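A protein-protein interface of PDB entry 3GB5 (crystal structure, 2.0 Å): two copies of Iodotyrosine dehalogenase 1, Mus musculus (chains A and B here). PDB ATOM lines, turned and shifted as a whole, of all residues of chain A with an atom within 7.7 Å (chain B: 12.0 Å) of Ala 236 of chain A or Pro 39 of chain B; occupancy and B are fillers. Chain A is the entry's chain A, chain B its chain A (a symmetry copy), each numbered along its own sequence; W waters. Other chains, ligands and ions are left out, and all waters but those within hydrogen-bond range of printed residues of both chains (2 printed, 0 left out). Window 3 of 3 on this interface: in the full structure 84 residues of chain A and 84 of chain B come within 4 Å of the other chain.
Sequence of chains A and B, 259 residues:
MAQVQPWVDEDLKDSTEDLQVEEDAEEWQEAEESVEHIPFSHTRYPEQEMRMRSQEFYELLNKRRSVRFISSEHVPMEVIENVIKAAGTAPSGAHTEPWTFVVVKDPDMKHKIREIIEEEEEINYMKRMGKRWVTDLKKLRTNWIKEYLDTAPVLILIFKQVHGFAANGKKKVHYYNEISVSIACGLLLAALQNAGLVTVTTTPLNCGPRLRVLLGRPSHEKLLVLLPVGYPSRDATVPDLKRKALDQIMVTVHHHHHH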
ATOM      1  N   ARG A  65      18.171  -5.113  -2.483  1.00  0.00           N
ATOM      2  CA  ARG A  65      18.398  -3.987  -1.550  1.00  0.00           C
ATOM      3  C   ARG A  65      19.689  -4.277  -0.786  1.00  0.00           C
ATOM      4  O   ARG A  65      20.009  -5.449  -0.554  1.00  0.00           O
ATOM      5  CB  ARG A  65      17.229  -3.799  -0.539  1.00  0.00           C
ATOM      6  CG  ARG A  65      15.862  -3.362  -1.160  1.00  0.00           C
ATOM      7  CD  ARG A  65      15.959  -1.993  -1.882  1.00  0.00           C
ATOM      8  NE  ARG A  65      16.491  -0.971  -0.984  1.00  0.00           N
ATOM      9  CZ  ARG A  65      15.762  -0.275  -0.116  1.00  0.00           C
ATOM     10  NH1 ARG A  65      14.433  -0.458  -0.046  1.00  0.00           N
ATOM     11  NH2 ARG A  65      16.363   0.625   0.675  1.00  0.00           N
ATOM     12  N   VAL A  67      21.545  -4.871   2.420  1.00  0.00           N
ATOM     13  CA  VAL A  67      20.958  -5.400   3.674  1.00  0.00           C
ATOM     14  C   VAL A  67      22.069  -5.432   4.717  1.00  0.00           C
ATOM     15  O   VAL A  67      23.110  -6.067   4.488  1.00  0.00           O
ATOM     16  CB  VAL A  67      20.374  -6.838   3.462  1.00  0.00           C
ATOM     17  CG1 VAL A  67      19.907  -7.492   4.874  1.00  0.00           C
ATOM     18  CG2 VAL A  67      19.197  -6.784   2.476  1.00  0.00           C
ATOM     19  N   ARG A  68      21.869  -4.772   5.846  1.00  0.00           N
ATOM     20  CA  ARG A  68      22.975  -4.655   6.814  1.00  0.00           C
ATOM     21  C   ARG A  68      22.755  -5.565   8.029  1.00  0.00           C
ATOM     22  O   ARG A  68      23.411  -5.390   9.076  1.00  0.00           O
ATOM     23  CB  ARG A  68      23.157  -3.179   7.255  1.00  0.00           C
ATOM     24  CG  ARG A  68      23.553  -2.264   6.048  1.00  0.00           C
ATOM     25  CD  ARG A  68      23.396  -0.757   6.350  1.00  0.00           C
ATOM     26  NE  ARG A  68      23.770   0.012   5.137  1.00  0.00           N
ATOM     27  CZ  ARG A  68      22.903   0.406   4.201  1.00  0.00           C
ATOM     28  NH1 ARG A  68      21.595   0.135   4.325  1.00  0.00           N
ATOM     29  NH2 ARG A  68      23.346   1.086   3.139  1.00  0.00           N
ATOM     30  N   PHE A  69      21.808  -6.488   7.892  1.00  0.00           N
ATOM     31  CA  PHE A  69      21.474  -7.444   8.949  1.00  0.00           C
ATOM     32  C   PHE A  69      21.512  -8.814   8.286  1.00  0.00           C
ATOM     33  O   PHE A  69      20.580  -9.190   7.589  1.00  0.00           O
ATOM     34  CB  PHE A  69      20.105  -7.127   9.555  1.00  0.00           C
ATOM     35  CG  PHE A  69      19.977  -5.692  10.034  1.00  0.00           C
ATOM     36  CD1 PHE A  69      20.472  -5.317  11.295  1.00  0.00           C
ATOM     37  CD2 PHE A  69      19.421  -4.700   9.187  1.00  0.00           C
ATOM     38  CE1 PHE A  69      20.366  -3.974  11.745  1.00  0.00           C
ATOM     39  CE2 PHE A  69      19.313  -3.355   9.619  1.00  0.00           C
ATOM     40  CZ  PHE A  69      19.784  -2.995  10.895  1.00  0.00           C
ATOM     41  N   ILE A  70      22.629  -9.506   8.457  1.00  0.00           N
ATOM     42  CA  ILE A  70      22.877 -10.751   7.720  1.00  0.00           C
ATOM     43  C   ILE A  70      22.954 -11.898   8.697  1.00  0.00           C
ATOM     44  O   ILE A  70      23.690 -11.854   9.728  1.00  0.00           O
ATOM     45  CB  ILE A  70      24.134 -10.625   6.822  1.00  0.00           C
ATOM     46  CG1 ILE A  70      23.885  -9.454   5.828  1.00  0.00           C
ATOM     47  CG2 ILE A  70      24.444 -11.943   6.082  1.00  0.00           C
ATOM     48  CD1 ILE A  70      25.116  -8.985   5.074  1.00  0.00           C
ATOM     49  N   SER A  71      22.150 -12.920   8.397  1.00  0.00           N
ATOM     50  CA  SER A  71      22.100 -14.144   9.223  1.00  0.00           C
ATOM     51  C   SER A  71      23.465 -14.859   9.220  1.00  0.00           C
ATOM     52  O   SER A  71      24.225 -14.769   8.225  1.00  0.00           O
ATOM     53  CB  SER A  71      21.018 -15.078   8.670  1.00  0.00           C
ATOM     54  OG  SER A  71      21.037 -16.341   9.339  1.00  0.00           O
ATOM     55  N   VAL A 198      22.026 -11.929  -0.136  1.00  0.00           N
ATOM     56  CA  VAL A 198      22.073 -10.490   0.025  1.00  0.00           C
ATOM     57  C   VAL A 198      23.437 -10.026   0.501  1.00  0.00           C
ATOM     58  O   VAL A 198      24.261 -10.810   1.019  1.00  0.00           O
ATOM     59  CB  VAL A 198      20.988  -9.941   1.023  1.00  0.00           C
ATOM     60  CG1 VAL A 198      19.534 -10.223   0.519  1.00  0.00           C
ATOM     61  CG2 VAL A 198      21.214 -10.472   2.476  1.00  0.00           C
ATOM     62  N   TYR A 231      22.188 -14.880   3.916  1.00  0.00           N
ATOM     63  CA  TYR A 231      20.778 -14.682   3.904  1.00  0.00           C
ATOM     64  C   TYR A 231      20.526 -13.461   4.787  1.00  0.00           C
ATOM     65  O   TYR A 231      21.264 -13.241   5.743  1.00  0.00           O
ATOM     66  CB  TYR A 231      20.028 -15.893   4.521  1.00  0.00           C
ATOM     67  CG  TYR A 231      20.233 -17.177   3.746  1.00  0.00           C
ATOM     68  CD1 TYR A 231      19.710 -17.332   2.448  1.00  0.00           C
ATOM     69  CD2 TYR A 231      20.956 -18.251   4.305  1.00  0.00           C
ATOM     70  CE1 TYR A 231      19.901 -18.557   1.729  1.00  0.00           C
ATOM     71  CE2 TYR A 231      21.164 -19.459   3.581  1.00  0.00           C
ATOM     72  CZ  TYR A 231      20.621 -19.588   2.300  1.00  0.00           C
ATOM     73  OH  TYR A 231      20.823 -20.747   1.577  1.00  0.00           O
ATOM     74  N   PRO A 232      19.455 -12.706   4.500  1.00  0.00           N
ATOM     75  CA  PRO A 232      19.095 -11.615   5.422  1.00  0.00           C
ATOM     76  C   PRO A 232      18.654 -12.161   6.785  1.00  0.00           C
ATOM     77  O   PRO A 232      18.033 -13.224   6.858  1.00  0.00           O
ATOM     78  CB  PRO A 232      17.899 -10.933   4.719  1.00  0.00           C
ATOM     79  CG  PRO A 232      17.256 -12.058   3.858  1.00  0.00           C
ATOM     80  CD  PRO A 232      18.511 -12.837   3.367  1.00  0.00           C
ATOM     81  N   SER A 233      18.966 -11.424   7.847  1.00  0.00           N
ATOM     82  CA  SER A 233      18.378 -11.665   9.172  1.00  0.00           C
ATOM     83  C   SER A 233      16.859 -11.855   9.055  1.00  0.00           C
ATOM     84  O   SER A 233      16.209 -11.198   8.239  1.00  0.00           O
ATOM     85  CB  SER A 233      18.664 -10.461  10.080  1.00  0.00           C
ATOM     86  OG  SER A 233      18.076 -10.613  11.359  1.00  0.00           O
ATOM     87  N   ARG A 234      16.298 -12.753   9.862  1.00  0.00           N
ATOM     88  CA  ARG A 234      14.853 -12.911   9.912  1.00  0.00           C
ATOM     89  C   ARG A 234      14.135 -11.605  10.304  1.00  0.00           C
ATOM     90  O   ARG A 234      12.962 -11.449   9.996  1.00  0.00           O
ATOM     91  CB  ARG A 234      14.467 -14.018  10.901  1.00  0.00           C
ATOM     92  CG  ARG A 234      14.852 -13.710  12.317  1.00  0.00           C
ATOM     93  CD  ARG A 234      14.633 -14.886  13.232  1.00  0.00           C
ATOM     94  NE  ARG A 234      15.072 -14.526  14.571  1.00  0.00           N
ATOM     95  CZ  ARG A 234      16.320 -14.667  15.021  1.00  0.00           C
ATOM     96  NH1 ARG A 234      17.286 -15.250  14.253  1.00  0.00           N
ATOM     97  NH2 ARG A 234      16.585 -14.267  16.262  1.00  0.00           N
ATOM     98  N   ASP A 235      14.819 -10.698  11.005  1.00  0.00           N
ATOM     99  CA  ASP A 235      14.215  -9.398  11.294  1.00  0.00           C
ATOM    100  C   ASP A 235      14.928  -8.229  10.573  1.00  0.00           C
ATOM    101  O   ASP A 235      14.876  -7.094  11.043  1.00  0.00           O
ATOM    102  CB  ASP A 235      14.158  -9.155  12.803  1.00  0.00           C
ATOM    103  CG  ASP A 235      15.446  -9.507  13.489  1.00  0.00           C
ATOM    104  OD1 ASP A 235      16.483  -9.622  12.793  1.00  0.00           O
ATOM    105  OD2 ASP A 235      15.397  -9.714  14.728  1.00  0.00           O
ATOM    106  N   ALA A 236      15.588  -8.520   9.451  1.00  0.00           N
ATOM    107  CA  ALA A 236      16.221  -7.468   8.654  1.00  0.00           C
ATOM    108  C   ALA A 236      15.245  -6.330   8.292  1.00  0.00           C
ATOM    109  O   ALA A 236      14.098  -6.550   7.908  1.00  0.00           O
ATOM    110  CB  ALA A 236      16.852  -8.030   7.377  1.00  0.00           C
ATOM    111  N   THR A 237      15.739  -5.107   8.387  1.00  0.00           N
ATOM    112  CA  THR A 237      15.016  -3.955   7.832  1.00  0.00           C
ATOM    113  C   THR A 237      15.902  -3.297   6.789  1.00  0.00           C
ATOM    114  O   THR A 237      17.077  -3.611   6.716  1.00  0.00           O
ATOM    115  CB  THR A 237      14.640  -2.923   8.930  1.00  0.00           C
ATOM    116  OG1 THR A 237      15.836  -2.425   9.536  1.00  0.00           O
ATOM    117  CG2 THR A 237      13.697  -3.531  10.017  1.00  0.00           C
ATOM    118  N   VAL A 238      15.316  -2.415   5.966  1.00  0.00           N
ATOM    119  CA  VAL A 238      16.039  -1.559   5.030  1.00  0.00           C
ATOM    120  C   VAL A 238      15.440  -0.141   5.157  1.00  0.00           C
ATOM    121  O   VAL A 238      14.270  -0.006   5.564  1.00  0.00           O
ATOM    122  CB  VAL A 238      15.929  -2.058   3.540  1.00  0.00           C
ATOM    123  CG1 VAL A 238      16.705  -3.412   3.326  1.00  0.00           C
ATOM    124  CG2 VAL A 238      14.466  -2.163   3.138  1.00  0.00           C
ATOM    125  N   PRO A 239      16.224   0.921   4.854  1.00  0.00           N
ATOM    126  CA  PRO A 239      15.566   2.242   4.862  1.00  0.00           C
ATOM    127  C   PRO A 239      14.551   2.308   3.717  1.00  0.00           C
ATOM    128  O   PRO A 239      14.727   1.640   2.678  1.00  0.00           O
ATOM    129  CB  PRO A 239      16.709   3.248   4.607  1.00  0.00           C
ATOM    130  CG  PRO A 239      17.859   2.454   4.156  1.00  0.00           C
ATOM    131  CD  PRO A 239      17.646   0.993   4.489  1.00  0.00           C
ATOM    132  N   GLU B  36      10.573   5.168   7.978  1.00  0.00           N
ATOM    133  CA  GLU B  36      11.982   5.391   7.596  1.00  0.00           C
ATOM    134  C   GLU B  36      12.604   4.027   7.332  1.00  0.00           C
ATOM    135  O   GLU B  36      13.203   3.868   6.314  1.00  0.00           O
ATOM    136  CB  GLU B  36      12.779   6.162   8.657  1.00  0.00           C
ATOM    137  CG  GLU B  36      14.115   6.778   8.170  1.00  0.00           C
ATOM    138  CD  GLU B  36      14.042   7.405   6.772  1.00  0.00           C
ATOM    139  OE1 GLU B  36      13.002   8.027   6.454  1.00  0.00           O
ATOM    140  OE2 GLU B  36      15.024   7.268   5.966  1.00  0.00           O
ATOM    141  N   HIS B  37      12.450   3.071   8.245  1.00  0.00           N
ATOM    142  CA  HIS B  37      12.911   1.687   8.020  1.00  0.00           C
ATOM    143  C   HIS B  37      11.732   0.740   7.967  1.00  0.00           C
ATOM    144  O   HIS B  37      10.776   0.890   8.720  1.00  0.00           O
ATOM    145  CB  HIS B  37      13.912   1.258   9.086  1.00  0.00           C
ATOM    146  CG  HIS B  37      15.092   2.177   9.170  1.00  0.00           C
ATOM    147  ND1 HIS B  37      16.255   1.964   8.460  1.00  0.00           N
ATOM    148  CD2 HIS B  37      15.260   3.351   9.832  1.00  0.00           C
ATOM    149  CE1 HIS B  37      17.102   2.949   8.701  1.00  0.00           C
ATOM    150  NE2 HIS B  37      16.523   3.804   9.529  1.00  0.00           N
ATOM    151  N   ILE B  38      11.787  -0.188   7.025  1.00  0.00           N
ATOM    152  CA  ILE B  38      10.694  -1.113   6.748  1.00  0.00           C
ATOM    153  C   ILE B  38      11.276  -2.551   6.764  1.00  0.00           C
ATOM    154  O   ILE B  38      12.463  -2.731   6.463  1.00  0.00           O
ATOM    155  CB  ILE B  38      10.005  -0.802   5.369  1.00  0.00           C
ATOM    156  CG1 ILE B  38      11.040  -0.738   4.243  1.00  0.00           C
ATOM    157  CG2 ILE B  38       9.189   0.524   5.456  1.00  0.00           C
ATOM    158  CD1 ILE B  38      10.526  -1.183   2.889  1.00  0.00           C
ATOM    159  N   PRO B  39      10.438  -3.561   7.087  1.00  0.00           N
ATOM    160  CA  PRO B  39      10.858  -4.966   6.971  1.00  0.00           C
ATOM    161  C   PRO B  39      11.313  -5.274   5.560  1.00  0.00           C
ATOM    162  O   PRO B  39      10.715  -4.788   4.581  1.00  0.00           O
ATOM    163  CB  PRO B  39       9.578  -5.749   7.289  1.00  0.00           C
ATOM    164  CG  PRO B  39       8.750  -4.817   8.107  1.00  0.00           C
ATOM    165  CD  PRO B  39       9.045  -3.445   7.560  1.00  0.00           C
ATOM    166  N   PHE B  40      12.399  -6.029   5.448  1.00  0.00           N
ATOM    167  CA  PHE B  40      12.931  -6.409   4.147  1.00  0.00           C
ATOM    168  C   PHE B  40      12.224  -7.683   3.668  1.00  0.00           C
ATOM    169  O   PHE B  40      12.134  -8.636   4.397  1.00  0.00           O
ATOM    170  CB  PHE B  40      14.451  -6.624   4.227  1.00  0.00           C
ATOM    171  CG  PHE B  40      15.054  -7.210   2.982  1.00  0.00           C
ATOM    172  CD1 PHE B  40      15.001  -6.518   1.777  1.00  0.00           C
ATOM    173  CD2 PHE B  40      15.674  -8.455   3.018  1.00  0.00           C
ATOM    174  CE1 PHE B  40      15.553  -7.033   0.644  1.00  0.00           C
ATOM    175  CE2 PHE B  40      16.245  -9.002   1.871  1.00  0.00           C
ATOM    176  CZ  PHE B  40      16.192  -8.290   0.675  1.00  0.00           C
ATOM    177  N   SER B  41      11.723  -7.648   2.432  1.00  0.00           N
ATOM    178  CA  SER B  41      11.041  -8.796   1.812  1.00  0.00           C
ATOM    179  C   SER B  41      12.017  -9.538   0.900  1.00  0.00           C
ATOM    180  O   SER B  41      12.601  -8.947  -0.028  1.00  0.00           O
ATOM    181  CB  SER B  41       9.793  -8.340   1.018  1.00  0.00           C
ATOM    182  OG  SER B  41      10.178  -7.778  -0.233  1.00  0.00           O
ATOM    183  N   HIS B  42      12.197 -10.826   1.169  1.00  0.00           N
ATOM    184  CA  HIS B  42      13.188 -11.614   0.437  1.00  0.00           C
ATOM    185  C   HIS B  42      12.719 -13.006  -0.027  1.00  0.00           C
ATOM    186  O   HIS B  42      12.201 -13.792   0.769  1.00  0.00           O
ATOM    187  CB  HIS B  42      14.433 -11.798   1.300  1.00  0.00           C
ATOM    188  CG  HIS B  42      15.575 -12.434   0.567  1.00  0.00           C
ATOM    189  ND1 HIS B  42      15.946 -13.749   0.762  1.00  0.00           N
ATOM    190  CD2 HIS B  42      16.418 -11.938  -0.373  1.00  0.00           C
ATOM    191  CE1 HIS B  42      16.986 -14.030  -0.005  1.00  0.00           C
ATOM    192  NE2 HIS B  42      17.288 -12.950  -0.709  1.00  0.00           N
ATOM    193  N   THR B  43      12.978 -13.316  -1.293  1.00  0.00           N
ATOM    194  CA  THR B  43      12.753 -14.656  -1.815  1.00  0.00           C
ATOM    195  C   THR B  43      13.945 -15.583  -1.505  1.00  0.00           C
ATOM    196  O   THR B  43      15.076 -15.283  -1.878  1.00  0.00           O
ATOM    197  CB  THR B  43      12.442 -14.610  -3.339  1.00  0.00           C
ATOM    198  OG1 THR B  43      11.301 -13.760  -3.532  1.00  0.00           O
ATOM    199  CG2 THR B  43      12.101 -16.006  -3.872  1.00  0.00           C
ATOM    200  N   ARG B  44      13.684 -16.667  -0.778  1.00  0.00           N
ATOM    201  CA  ARG B  44      14.700 -17.714  -0.561  1.00  0.00           C
ATOM    202  C   ARG B  44      14.382 -18.956  -1.412  1.00  0.00           C
ATOM    203  O   ARG B  44      13.265 -19.455  -1.387  1.00  0.00           O
ATOM    204  CB  ARG B  44      14.820 -18.070   0.931  1.00  0.00           C
ATOM    205  CG  ARG B  44      15.882 -19.087   1.224  1.00  0.00           C
ATOM    206  CD  ARG B  44      16.241 -19.153   2.690  1.00  0.00           C
ATOM    207  NE  ARG B  44      17.053 -20.338   2.961  1.00  0.00           N
ATOM    208  CZ  ARG B  44      17.700 -20.569   4.098  1.00  0.00           C
ATOM    209  NH1 ARG B  44      17.628 -19.689   5.083  1.00  0.00           N
ATOM    210  NH2 ARG B  44      18.408 -21.697   4.252  1.00  0.00           N
HETATM  211  O   HOH W   1      18.154 -22.050   0.902  1.00  0.00           O
HETATM  212  O   HOH W   2      17.131  -0.383   8.048  1.00  0.00           O
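O of Ala 236 of chain A lies within hydrogen-bond range of N of Phe 40 of chain B, 3.0 Å away.
The backbone carbonyl oxygen (O) of Val 238 of chain A lies within hydrogen-bond range of the backbone NH (N) of Ile 38 of chain B (2.9 Å).
The backbone carbonyl oxygen of Pro 239 of chain A sits at hydrogen-bond distance from the guanidinium group of Arg 65 of chain A, 2.8 Å away.
N of Ser 71 of chain A is in hydrogen-bond range of O of Tyr 231 of chain A, at 2.8 Å.
CE1 of Phe 40 of chain B touches CB of Arg 65 of chain A (3.8 Å).
CG1 of Val 198 of chain A touches CD2 of His 42 of chain B, 3.7 Å away.
Tyr 231 of chain A touches Arg 44 of chain B.
Pro 232 of chain A touches Phe 40 of chain B.
His 42 of chain B touches Pro 232 of chain A.
Ala 236 of chain A touches Pro 39 of chain B.
Ile 38 of chain B touches Thr 237 of chain A (O to CA, 3.1 Å).
CA of His 37 of chain B touches O of Val 238 of chain A (3.3 Å).
CD1 of Phe 40 of chain B touches CG1 of Val 238 of chain A, at 3.9 Å.
Pro 239 of chain A touches His 37 of chain B (CA to ND1, 3.7 Å).
Of chain B, only Phe 40 (3.7 Å) comes within 4 Å of Val 67 of chain A.
No residue of chain B comes within 4 Å of Phe 69 of chain A.
Printed residues of chain B within 4 Å of Pro 232 of chain A: Phe 40 (3.7 Å) and His 42 (3.7 Å).
Thr 237 of chain A touches one residue of chain B.
Of the printed residues of chain A, His 37 of chain B touches Val 238 and Pro 239.
Printed residues of chain A within 4 Å of Ile 38 of chain B: Thr 237 (3.1 Å) and Val 238 (2.9 Å).
Pro 39 of chain B touches just one residue of chain A: Ala 236.
Of the printed residues of chain A, His 42 of chain B touches Val 198 (3.7 Å) and Pro 232 (3.7 Å).
Of the printed residues of chain A, Arg 44 of chain B touches Tyr 231 (3.6 Å).
The nearest printed residue of chain B that does not touch Val 198 of chain A is Ser 41 of chain B (7.1 Å).
Hydrophobic or aromatic side chains of chain A that line the printed part of chain B: Val 67, Val 198, Tyr 231, Pro 232, Val 238 and Pro 239.
Among the printed residues, no Asp or Glu carboxylate lies within 4 Å of a Lys or Arg side-chain nitrogen of the other chain.
No position is printed for both chains.
Water W2 lies within hydrogen-bond range of a ring nitrogen (ND1) of His 37 of chain B (2.5 Å), the side-chain hydroxyl of Thr 237 of chain A (2.8 Å) and the backbone NH of Val 238 of chain A (3.4 Å).
Water W1 bridges the guanidinium group of Arg 44 of chain B and the side-chain hydroxyl of Tyr 231 of chain A.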
